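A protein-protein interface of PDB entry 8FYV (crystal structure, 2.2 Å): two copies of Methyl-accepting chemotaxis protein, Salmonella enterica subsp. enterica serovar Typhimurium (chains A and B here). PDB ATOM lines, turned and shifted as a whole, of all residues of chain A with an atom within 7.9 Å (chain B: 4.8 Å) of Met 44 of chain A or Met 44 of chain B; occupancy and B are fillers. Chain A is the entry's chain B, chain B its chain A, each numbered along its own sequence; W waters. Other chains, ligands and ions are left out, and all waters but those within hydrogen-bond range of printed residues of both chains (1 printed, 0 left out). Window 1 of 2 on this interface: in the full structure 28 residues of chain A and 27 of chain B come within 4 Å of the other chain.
O of Ile 50 of chain B lies close to OD1 of Asn 118 of chain A (3.4 Å).
O of Met 45 of chain B sits at hydrogen-bond distance from OG of Ser 48 of chain B (3.2 Å).
The backbone carbonyl oxygen (O) of Met 45 of chain B lies within hydrogen-bond range of the backbone NH (N) of Ile 50 of chain B (3.1 Å).
The backbone carbonyl oxygen (O) of Met 44 of chain A is in hydrogen-bond range of the side-chain hydroxyl (OG) of Ser 48 of chain A, 3.0 Å away.
O of Met 45 of chain A sits at hydrogen-bond distance from N of Ile 50 of chain A.
Among the printed residues, pairs that only touch across the chains: Gly 40 of chain A with Ile 41 of chain B, Ile 41 of chain A with Gly 40 of chain B, Ile 41 of chain A with Ile 41 of chain B, Met 44 of chain A with Met 44 of chain B, Met 44 of chain A with Met 45 of chain B, Met 44 of chain A with Ser 48 of chain B, Met 45 of chain A with Ile 117 of chain B, Ile 50 of chain A with Met 44 of chain B, Ile 50 of chain A with Ile 117 of chain B, Ile 117 of chain A with Met 45 of chain B and Asn 118 of chain A with Met 45 of chain B.
Met 44 of chain A touches three residues of chain B.
Printed residues of chain B within 4 Å of Met 45 of chain A: Ile 117.
Asp 46 of chain A touches none of the printed residues of chain B.
Asn 49 of chain A touches none of the printed residues of chain B.
Of the printed residues of chain A, Ile 41 of chain B touches Gly 40 (3.9 Å) and Ile 41 (3.5 Å).
Of the printed residues of chain A, Met 45 of chain B touches Met 44, Ile 117 and Asn 118.
Of the printed residues of chain A, Ser 48 of chain B touches Met 44 (3.7 Å).
Printed residues of chain A within 4 Å of Ile 50 of chain B: Asn 118.
The nearest residue of chain B that does not touch Met 44 of chain A is Ile 50 of chain B (4.1 Å).
The nearest printed residue of chain B that does not touch Gly 40 of chain A is Met 44 of chain B (5.9 Å).
Printed residues of chain B that touch a printed residue of chain A: Gly 40, Ile 41, Met 44, Met 45, Ser 48, Ile 50 and Ile 117.
Hydrophobic or aromatic side chains of chain B that line the printed part of chain A: Ile 41, Met 44, Met 45 and Ile 117.
Hydrophobic or aromatic side chains of chain A that line the printed part of chain B: Ile 41, Met 44, Met 45, Ile 50 and Ile 117.
Among the printed residues, no Asp or Glu carboxylate lies within 4 Å of a Lys or Arg side-chain nitrogen of the other chain.
Met 44 of chain A touches its own counterpart, Met 44 of chain B.
Met 44 of chain A touches Ser 48 of chain B, but with the chains exchanged Ser 48 of chain A does not touch Met 44 of chain B (4.2 Å).
Ile 50 of chain A touches Met 44 of chain B, but with the chains exchanged Met 44 of chain A does not touch Ile 50 of chain B (4.1 Å).
Ile 50 of chain A touches Ile 117 of chain B, but with the chains exchanged Ile 117 of chain A does not touch Ile 50 of chain B (4.4 Å).
Positions printed for both chains: 40, 41, 42, 43, 44, 45, 46, 47, 48, 50 and 117.
Water W1 lies within hydrogen-bond range of the side-chain hydroxyl (OG) of Ser 48 of chain A (3.0 Å), the backbone carbonyl oxygen (O) of Met 44 of chain B (3.1 Å) and the side-chain hydroxyl (OG) of Ser 48 of chain B (3.4 Å).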
ATOM      1  N   ARG A  38      -5.100  -8.513   9.927  1.00  0.00           N
ATOM      2  CA  ARG A  38      -3.646  -8.496  10.039  1.00  0.00           C
ATOM      3  C   ARG A  38      -3.038  -7.504   9.056  1.00  0.00           C
ATOM      4  O   ARG A  38      -2.110  -6.761   9.401  1.00  0.00           O
ATOM      5  CB  ARG A  38      -3.078  -9.893   9.793  1.00  0.00           C
ATOM      6  CG  ARG A  38      -3.244 -10.854  10.951  1.00  0.00           C
ATOM      7  CD  ARG A  38      -2.610 -12.196  10.628  1.00  0.00           C
ATOM      8  NE  ARG A  38      -1.153 -12.118  10.588  1.00  0.00           N
ATOM      9  CZ  ARG A  38      -0.372 -12.978   9.947  1.00  0.00           C
ATOM     10  NH1 ARG A  38      -0.874 -13.992   9.262  1.00  0.00           N
ATOM     11  NH2 ARG A  38       0.947 -12.815   9.995  1.00  0.00           N
ATOM     12  N   ALA A  39      -3.545  -7.480   7.821  1.00  0.00           N
ATOM     13  CA  ALA A  39      -3.029  -6.545   6.825  1.00  0.00           C
ATOM     14  C   ALA A  39      -3.293  -5.102   7.237  1.00  0.00           C
ATOM     15  O   ALA A  39      -2.467  -4.215   6.988  1.00  0.00           O
ATOM     16  CB  ALA A  39      -3.655  -6.838   5.462  1.00  0.00           C
ATOM     17  N   GLY A  40      -4.440  -4.846   7.868  1.00  0.00           N
ATOM     18  CA  GLY A  40      -4.734  -3.495   8.318  1.00  0.00           C
ATOM     19  C   GLY A  40      -3.723  -2.985   9.325  1.00  0.00           C
ATOM     20  O   GLY A  40      -3.337  -1.813   9.294  1.00  0.00           O
ATOM     21  N   ILE A  41      -3.281  -3.856  10.236  1.00  0.00           N
ATOM     22  CA  ILE A  41      -2.279  -3.457  11.222  1.00  0.00           C
ATOM     23  C   ILE A  41      -0.969  -3.110  10.528  1.00  0.00           C
ATOM     24  O   ILE A  41      -0.378  -2.050  10.769  1.00  0.00           O
ATOM     25  CB  ILE A  41      -2.075  -4.566  12.270  1.00  0.00           C
ATOM     26  CG1 ILE A  41      -3.392  -4.902  12.967  1.00  0.00           C
ATOM     27  CG2 ILE A  41      -1.031  -4.136  13.296  1.00  0.00           C
ATOM     28  CD1 ILE A  41      -3.304  -6.107  13.886  1.00  0.00           C
ATOM     29  N   ARG A  42      -0.483  -4.008   9.668  1.00  0.00           N
ATOM     30  CA  ARG A  42       0.773  -3.748   8.971  1.00  0.00           C
ATOM     31  C   ARG A  42       0.675  -2.487   8.123  1.00  0.00           C
ATOM     32  O   ARG A  42       1.628  -1.703   8.054  1.00  0.00           O
ATOM     33  CB  ARG A  42       1.157  -4.950   8.107  1.00  0.00           C
ATOM     34  CG  ARG A  42       2.486  -4.801   7.363  1.00  0.00           C
ATOM     35  CD  ARG A  42       3.683  -4.749   8.307  1.00  0.00           C
ATOM     36  NE  ARG A  42       4.838  -4.105   7.688  1.00  0.00           N
ATOM     37  CZ  ARG A  42       5.885  -4.746   7.184  1.00  0.00           C
ATOM     38  NH1 ARG A  42       5.974  -6.066   7.217  1.00  0.00           N
ATOM     39  NH2 ARG A  42       6.872  -4.043   6.635  1.00  0.00           N
ATOM     40  N   TRP A  43      -0.470  -2.273   7.469  1.00  0.00           N
ATOM     41  CA  TRP A  43      -0.669  -1.037   6.718  1.00  0.00           C
ATOM     42  C   TRP A  43      -0.429   0.174   7.609  1.00  0.00           C
ATOM     43  O   TRP A  43       0.313   1.093   7.246  1.00  0.00           O
ATOM     44  CB  TRP A  43      -2.079  -1.001   6.124  1.00  0.00           C
ATOM     45  CG  TRP A  43      -2.291   0.124   5.153  1.00  0.00           C
ATOM     46  CD1 TRP A  43      -2.154   0.074   3.795  1.00  0.00           C
ATOM     47  CD2 TRP A  43      -2.676   1.469   5.466  1.00  0.00           C
ATOM     48  NE1 TRP A  43      -2.429   1.303   3.244  1.00  0.00           N
ATOM     49  CE2 TRP A  43      -2.753   2.176   4.248  1.00  0.00           C
ATOM     50  CE3 TRP A  43      -2.967   2.142   6.656  1.00  0.00           C
ATOM     51  CZ2 TRP A  43      -3.105   3.523   4.188  1.00  0.00           C
ATOM     52  CZ3 TRP A  43      -3.316   3.479   6.594  1.00  0.00           C
ATOM     53  CH2 TRP A  43      -3.383   4.155   5.369  1.00  0.00           C
ATOM     54  N   MET A  44      -1.041   0.181   8.795  1.00  0.00           N
ATOM     55  CA  MET A  44      -0.826   1.282   9.729  1.00  0.00           C
ATOM     56  C   MET A  44       0.612   1.320  10.228  1.00  0.00           C
ATOM     57  O   MET A  44       1.158   2.405  10.461  1.00  0.00           O
ATOM     58  CB  MET A  44      -1.799   1.163  10.900  1.00  0.00           C
ATOM     59  CG  MET A  44      -3.247   1.436  10.512  1.00  0.00           C
ATOM     60  SD  MET A  44      -3.718   3.179  10.564  1.00  0.00           S
ATOM     61  CE  MET A  44      -3.115   3.711  12.172  1.00  0.00           C
ATOM     62  N   MET A  45       1.240   0.154  10.395  1.00  0.00           N
ATOM     63  CA  MET A  45       2.641   0.115  10.798  1.00  0.00           C
ATOM     64  C   MET A  45       3.531   0.764   9.746  1.00  0.00           C
ATOM     65  O   MET A  45       4.474   1.493  10.080  1.00  0.00           O
ATOM     66  CB  MET A  45       3.073  -1.333  11.036  1.00  0.00           C
ATOM     67  CG  MET A  45       2.456  -1.985  12.264  1.00  0.00           C
ATOM     68  SD  MET A  45       3.075  -3.659  12.536  1.00  0.00           S
ATOM     69  CE  MET A  45       3.357  -3.623  14.303  1.00  0.00           C
ATOM     70  N   ASP A  46       3.249   0.504   8.467  1.00  0.00           N
ATOM     71  CA  ASP A  46       4.050   1.091   7.397  1.00  0.00           C
ATOM     72  C   ASP A  46       3.916   2.609   7.377  1.00  0.00           C
ATOM     73  O   ASP A  46       4.906   3.325   7.183  1.00  0.00           O
ATOM     74  CB  ASP A  46       3.632   0.497   6.052  1.00  0.00           C
ATOM     75  CG  ASP A  46       4.167  -0.908   5.844  1.00  0.00           C
ATOM     76  OD1 ASP A  46       3.622  -1.634   4.985  1.00  0.00           O
ATOM     77  OD2 ASP A  46       5.136  -1.287   6.535  1.00  0.00           O
ATOM     78  N   GLN A  47       2.699   3.121   7.576  1.00  0.00           N
ATOM     79  CA  GLN A  47       2.502   4.566   7.598  1.00  0.00           C
ATOM     80  C   GLN A  47       3.195   5.226   8.784  1.00  0.00           C
ATOM     81  O   GLN A  47       3.493   6.423   8.722  1.00  0.00           O
ATOM     82  CB  GLN A  47       1.008   4.895   7.623  1.00  0.00           C
ATOM     83  CG  GLN A  47       0.231   4.379   6.419  1.00  0.00           C
ATOM     84  CD  GLN A  47       0.774   4.896   5.096  1.00  0.00           C
ATOM     85  OE1 GLN A  47       1.551   4.217   4.425  1.00  0.00           O
ATOM     86  NE2 GLN A  47       0.365   6.101   4.715  1.00  0.00           N
ATOM     87  N   SER A  48       3.462   4.478   9.854  1.00  0.00           N
ATOM     88  CA  SER A  48       4.167   4.998  11.020  1.00  0.00           C
ATOM     89  C   SER A  48       5.634   4.584  11.057  1.00  0.00           C
ATOM     90  O   SER A  48       6.328   4.898  12.029  1.00  0.00           O
ATOM     91  CB  SER A  48       3.471   4.534  12.305  1.00  0.00           C
ATOM     92  OG  SER A  48       2.064   4.676  12.207  1.00  0.00           O
ATOM     93  N   ASN A  49       6.116   3.880  10.031  1.00  0.00           N
ATOM     94  CA  ASN A  49       7.527   3.503   9.920  1.00  0.00           C
ATOM     95  C   ASN A  49       7.960   2.579  11.058  1.00  0.00           C
ATOM     96  O   ASN A  49       9.053   2.716  11.612  1.00  0.00           O
ATOM     97  CB  ASN A  49       8.423   4.743   9.864  1.00  0.00           C
ATOM     98  CG  ASN A  49       8.356   5.453   8.523  1.00  0.00           C
ATOM     99  OD1 ASN A  49       7.659   5.014   7.609  1.00  0.00           O
ATOM    100  ND2 ASN A  49       9.080   6.558   8.403  1.00  0.00           N
ATOM    101  N   ILE A  50       7.103   1.620  11.405  1.00  0.00           N
ATOM    102  CA  ILE A  50       7.462   0.587  12.371  1.00  0.00           C
ATOM    103  C   ILE A  50       6.992  -0.764  11.843  1.00  0.00           C
ATOM    104  O   ILE A  50       6.515  -1.612  12.606  1.00  0.00           O
ATOM    105  CB  ILE A  50       6.873   0.878  13.766  1.00  0.00           C
ATOM    106  CG1 ILE A  50       5.344   0.934  13.722  1.00  0.00           C
ATOM    107  CG2 ILE A  50       7.427   2.187  14.314  1.00  0.00           C
ATOM    108  CD1 ILE A  50       4.671   0.339  14.952  1.00  0.00           C
ATOM    109  N   GLY A  51       7.131  -0.972  10.536  1.00  0.00           N
ATOM    110  CA  GLY A  51       6.647  -2.202   9.932  1.00  0.00           C
ATOM    111  C   GLY A  51       7.542  -3.385  10.261  1.00  0.00           C
ATOM    112  O   GLY A  51       8.770  -3.282  10.278  1.00  0.00           O
ATOM    113  N   VAL A  56       2.046  -6.236   4.024  1.00  0.00           N
ATOM    114  CA  VAL A  56       0.704  -6.016   3.493  1.00  0.00           C
ATOM    115  C   VAL A  56       0.481  -6.850   2.238  1.00  0.00           C
ATOM    116  O   VAL A  56      -0.576  -7.469   2.067  1.00  0.00           O
ATOM    117  CB  VAL A  56       0.484  -4.517   3.209  1.00  0.00           C
ATOM    118  CG1 VAL A  56      -0.833  -4.300   2.466  1.00  0.00           C
ATOM    119  CG2 VAL A  56       0.517  -3.717   4.500  1.00  0.00           C
ATOM    120  N   LEU A 112      -8.773  -1.552   1.565  1.00  0.00           N
ATOM    121  CA  LEU A 112      -7.413  -1.566   2.086  1.00  0.00           C
ATOM    122  C   LEU A 112      -6.400  -1.305   0.978  1.00  0.00           C
ATOM    123  O   LEU A 112      -5.405  -0.604   1.193  1.00  0.00           O
ATOM    124  CB  LEU A 112      -7.134  -2.896   2.783  1.00  0.00           C
ATOM    125  CG  LEU A 112      -5.914  -2.921   3.707  1.00  0.00           C
ATOM    126  CD1 LEU A 112      -6.022  -1.875   4.808  1.00  0.00           C
ATOM    127  CD2 LEU A 112      -5.738  -4.304   4.305  1.00  0.00           C
ATOM    128  N   ILE A 117      -8.439   3.277   5.431  1.00  0.00           N
ATOM    129  CA  ILE A 117      -8.378   2.502   6.665  1.00  0.00           C
ATOM    130  C   ILE A 117      -9.604   2.755   7.537  1.00  0.00           C
ATOM    131  O   ILE A 117     -10.049   1.858   8.264  1.00  0.00           O
ATOM    132  CB  ILE A 117      -7.067   2.812   7.414  1.00  0.00           C
ATOM    133  CG1 ILE A 117      -6.834   1.790   8.532  1.00  0.00           C
ATOM    134  CG2 ILE A 117      -7.080   4.236   7.968  1.00  0.00           C
ATOM    135  CD1 ILE A 117      -6.453   0.403   8.036  1.00  0.00           C
ATOM    136  N   ASN A 118     -10.173   3.962   7.482  1.00  0.00           N
ATOM    137  CA  ASN A 118     -11.340   4.266   8.307  1.00  0.00           C
ATOM    138  C   ASN A 118     -12.580   3.543   7.792  1.00  0.00           C
ATOM    139  O   ASN A 118     -13.295   2.892   8.563  1.00  0.00           O
ATOM    140  CB  ASN A 118     -11.573   5.776   8.351  1.00  0.00           C
ATOM    141  CG  ASN A 118     -10.435   6.520   9.024  1.00  0.00           C
ATOM    142  OD1 ASN A 118     -10.194   6.357  10.220  1.00  0.00           O
ATOM    143  ND2 ASN A 118      -9.727   7.339   8.256  1.00  0.00           N
ATOM    144  N   GLY B  40      -5.814  -4.554  17.400  1.00  0.00           N
ATOM    145  CA  GLY B  40      -4.520  -4.052  16.968  1.00  0.00           C
ATOM    146  C   GLY B  40      -4.636  -2.862  16.037  1.00  0.00           C
ATOM    147  O   GLY B  40      -3.854  -1.910  16.127  1.00  0.00           O
ATOM    148  N   ILE B  41      -5.609  -2.898  15.123  1.00  0.00           N
ATOM    149  CA  ILE B  41      -5.827  -1.767  14.226  1.00  0.00           C
ATOM    150  C   ILE B  41      -6.249  -0.538  15.023  1.00  0.00           C
ATOM    151  O   ILE B  41      -5.695   0.554  14.857  1.00  0.00           O
ATOM    152  CB  ILE B  41      -6.870  -2.124  13.151  1.00  0.00           C
ATOM    153  CG1 ILE B  41      -6.378  -3.301  12.307  1.00  0.00           C
ATOM    154  CG2 ILE B  41      -7.167  -0.913  12.262  1.00  0.00           C
ATOM    155  CD1 ILE B  41      -7.364  -3.761  11.250  1.00  0.00           C
ATOM    156  N   ARG B  42      -7.247  -0.700  15.896  1.00  0.00           N
ATOM    157  CA  ARG B  42      -7.706   0.428  16.703  1.00  0.00           C
ATOM    158  C   ARG B  42      -6.575   0.978  17.558  1.00  0.00           C
ATOM    159  O   ARG B  42      -6.392   2.197  17.649  1.00  0.00           O
ATOM    160  CB  ARG B  42      -8.885   0.007  17.580  1.00  0.00           C
ATOM    161  CG  ARG B  42      -9.492   1.142  18.410  1.00  0.00           C
ATOM    162  CD  ARG B  42     -10.098   2.243  17.541  1.00  0.00           C
ATOM    163  NE  ARG B  42     -10.126   3.532  18.227  1.00  0.00           N
ATOM    164  CZ  ARG B  42     -11.214   4.094  18.743  1.00  0.00           C
ATOM    165  NH1 ARG B  42     -12.397   3.506  18.677  1.00  0.00           N
ATOM    166  NH2 ARG B  42     -11.110   5.279  19.339  1.00  0.00           N
ATOM    167  N   TRP B  43      -5.807   0.095  18.199  1.00  0.00           N
ATOM    168  CA  TRP B  43      -4.640   0.546  18.947  1.00  0.00           C
ATOM    169  C   TRP B  43      -3.735   1.390  18.058  1.00  0.00           C
ATOM    170  O   TRP B  43      -3.333   2.497  18.429  1.00  0.00           O
ATOM    171  CB  TRP B  43      -3.885  -0.657  19.514  1.00  0.00           C
ATOM    172  CG  TRP B  43      -2.790  -0.285  20.466  1.00  0.00           C
ATOM    173  CD1 TRP B  43      -2.862  -0.256  21.829  1.00  0.00           C
ATOM    174  CD2 TRP B  43      -1.456   0.111  20.127  1.00  0.00           C
ATOM    175  NE1 TRP B  43      -1.656   0.135  22.359  1.00  0.00           N
ATOM    176  CE2 TRP B  43      -0.776   0.366  21.334  1.00  0.00           C
ATOM    177  CE3 TRP B  43      -0.771   0.274  18.919  1.00  0.00           C
ATOM    178  CZ2 TRP B  43       0.556   0.776  21.368  1.00  0.00           C
ATOM    179  CZ3 TRP B  43       0.550   0.681  18.955  1.00  0.00           C
ATOM    180  CH2 TRP B  43       1.199   0.928  20.171  1.00  0.00           C
ATOM    181  N   MET B  44      -3.430   0.885  16.861  1.00  0.00           N
ATOM    182  CA  MET B  44      -2.621   1.642  15.912  1.00  0.00           C
ATOM    183  C   MET B  44      -3.266   2.986  15.595  1.00  0.00           C
ATOM    184  O   MET B  44      -2.594   4.023  15.567  1.00  0.00           O
ATOM    185  CB  MET B  44      -2.427   0.824  14.635  1.00  0.00           C
ATOM    186  CG  MET B  44      -1.015   0.824  14.091  1.00  0.00           C
ATOM    187  SD  MET B  44       0.215   0.310  15.299  1.00  0.00           S
ATOM    188  CE  MET B  44       1.568   1.392  14.852  1.00  0.00           C
ATOM    189  N   MET B  45      -4.578   2.985  15.347  1.00  0.00           N
ATOM    190  CA  MET B  45      -5.277   4.231  15.053  1.00  0.00           C
ATOM    191  C   MET B  45      -5.149   5.220  16.203  1.00  0.00           C
ATOM    192  O   MET B  45      -4.903   6.412  15.984  1.00  0.00           O
ATOM    193  CB  MET B  45      -6.750   3.943  14.767  1.00  0.00           C
ATOM    194  CG  MET B  45      -7.007   3.297  13.422  1.00  0.00           C
ATOM    195  SD  MET B  45      -8.764   3.020  13.142  1.00  0.00           S
ATOM    196  CE  MET B  45      -8.793   2.807  11.364  1.00  0.00           C
ATOM    197  N   ASP B  46      -5.313   4.743  17.440  1.00  0.00           N
ATOM    198  CA  ASP B  46      -5.250   5.635  18.592  1.00  0.00           C
ATOM    199  C   ASP B  46      -3.899   6.330  18.693  1.00  0.00           C
ATOM    200  O   ASP B  46      -3.825   7.471  19.163  1.00  0.00           O
ATOM    201  CB  ASP B  46      -5.539   4.854  19.875  1.00  0.00           C
ATOM    202  CG  ASP B  46      -7.003   4.478  20.014  1.00  0.00           C
ATOM    203  OD1 ASP B  46      -7.336   3.693  20.930  1.00  0.00           O
ATOM    204  OD2 ASP B  46      -7.821   4.966  19.207  1.00  0.00           O
ATOM    205  N   GLN B  47      -2.824   5.665  18.266  1.00  0.00           N
ATOM    206  CA  GLN B  47      -1.505   6.287  18.334  1.00  0.00           C
ATOM    207  C   GLN B  47      -1.448   7.544  17.476  1.00  0.00           C
ATOM    208  O   GLN B  47      -0.785   8.523  17.840  1.00  0.00           O
ATOM    209  CB  GLN B  47      -0.429   5.293  17.896  1.00  0.00           C
ATOM    210  CG  GLN B  47      -0.457   3.973  18.645  1.00  0.00           C
ATOM    211  CD  GLN B  47      -0.371   4.152  20.148  1.00  0.00           C
ATOM    212  OE1 GLN B  47      -1.250   3.708  20.888  1.00  0.00           O
ATOM    213  NE2 GLN B  47       0.691   4.802  20.607  1.00  0.00           N
ATOM    214  N   SER B  48      -2.135   7.537  16.334  1.00  0.00           N
ATOM    215  CA  SER B  48      -2.186   8.686  15.442  1.00  0.00           C
ATOM    216  C   SER B  48      -3.476   9.482  15.588  1.00  0.00           C
ATOM    217  O   SER B  48      -3.750  10.356  14.760  1.00  0.00           O
ATOM    218  CB  SER B  48      -2.013   8.232  13.989  1.00  0.00           C
ATOM    219  OG  SER B  48      -2.841   7.120  13.696  1.00  0.00           O
ATOM    220  N   ILE B  50      -6.708   8.835  15.122  1.00  0.00           N
ATOM    221  CA  ILE B  50      -7.668   8.725  14.030  1.00  0.00           C
ATOM    222  C   ILE B  50      -8.632   7.585  14.338  1.00  0.00           C
ATOM    223  O   ILE B  50      -9.299   7.059  13.440  1.00  0.00           O
ATOM    224  CB  ILE B  50      -6.959   8.515  12.679  1.00  0.00           C
ATOM    225  CG1 ILE B  50      -6.318   7.128  12.603  1.00  0.00           C
ATOM    226  CG2 ILE B  50      -5.900   9.595  12.462  1.00  0.00           C
ATOM    227  CD1 ILE B  50      -5.653   6.838  11.271  1.00  0.00           C
ATOM    228  N   ILE B 117       3.143  -3.664  20.317  1.00  0.00           N
ATOM    229  CA  ILE B 117       2.461  -3.877  19.043  1.00  0.00           C
ATOM    230  C   ILE B 117       3.323  -4.706  18.099  1.00  0.00           C
ATOM    231  O   ILE B 117       2.814  -5.569  17.374  1.00  0.00           O
ATOM    232  CB  ILE B 117       2.069  -2.523  18.424  1.00  0.00           C
ATOM    233  CG1 ILE B 117       1.098  -2.722  17.255  1.00  0.00           C
ATOM    234  CG2 ILE B 117       3.306  -1.769  17.961  1.00  0.00           C
ATOM    235  CD1 ILE B 117      -0.191  -3.441  17.623  1.00  0.00           C
HETATM  236  O   HOH W   1      -0.108   5.218  14.263  1.00  0.00           O
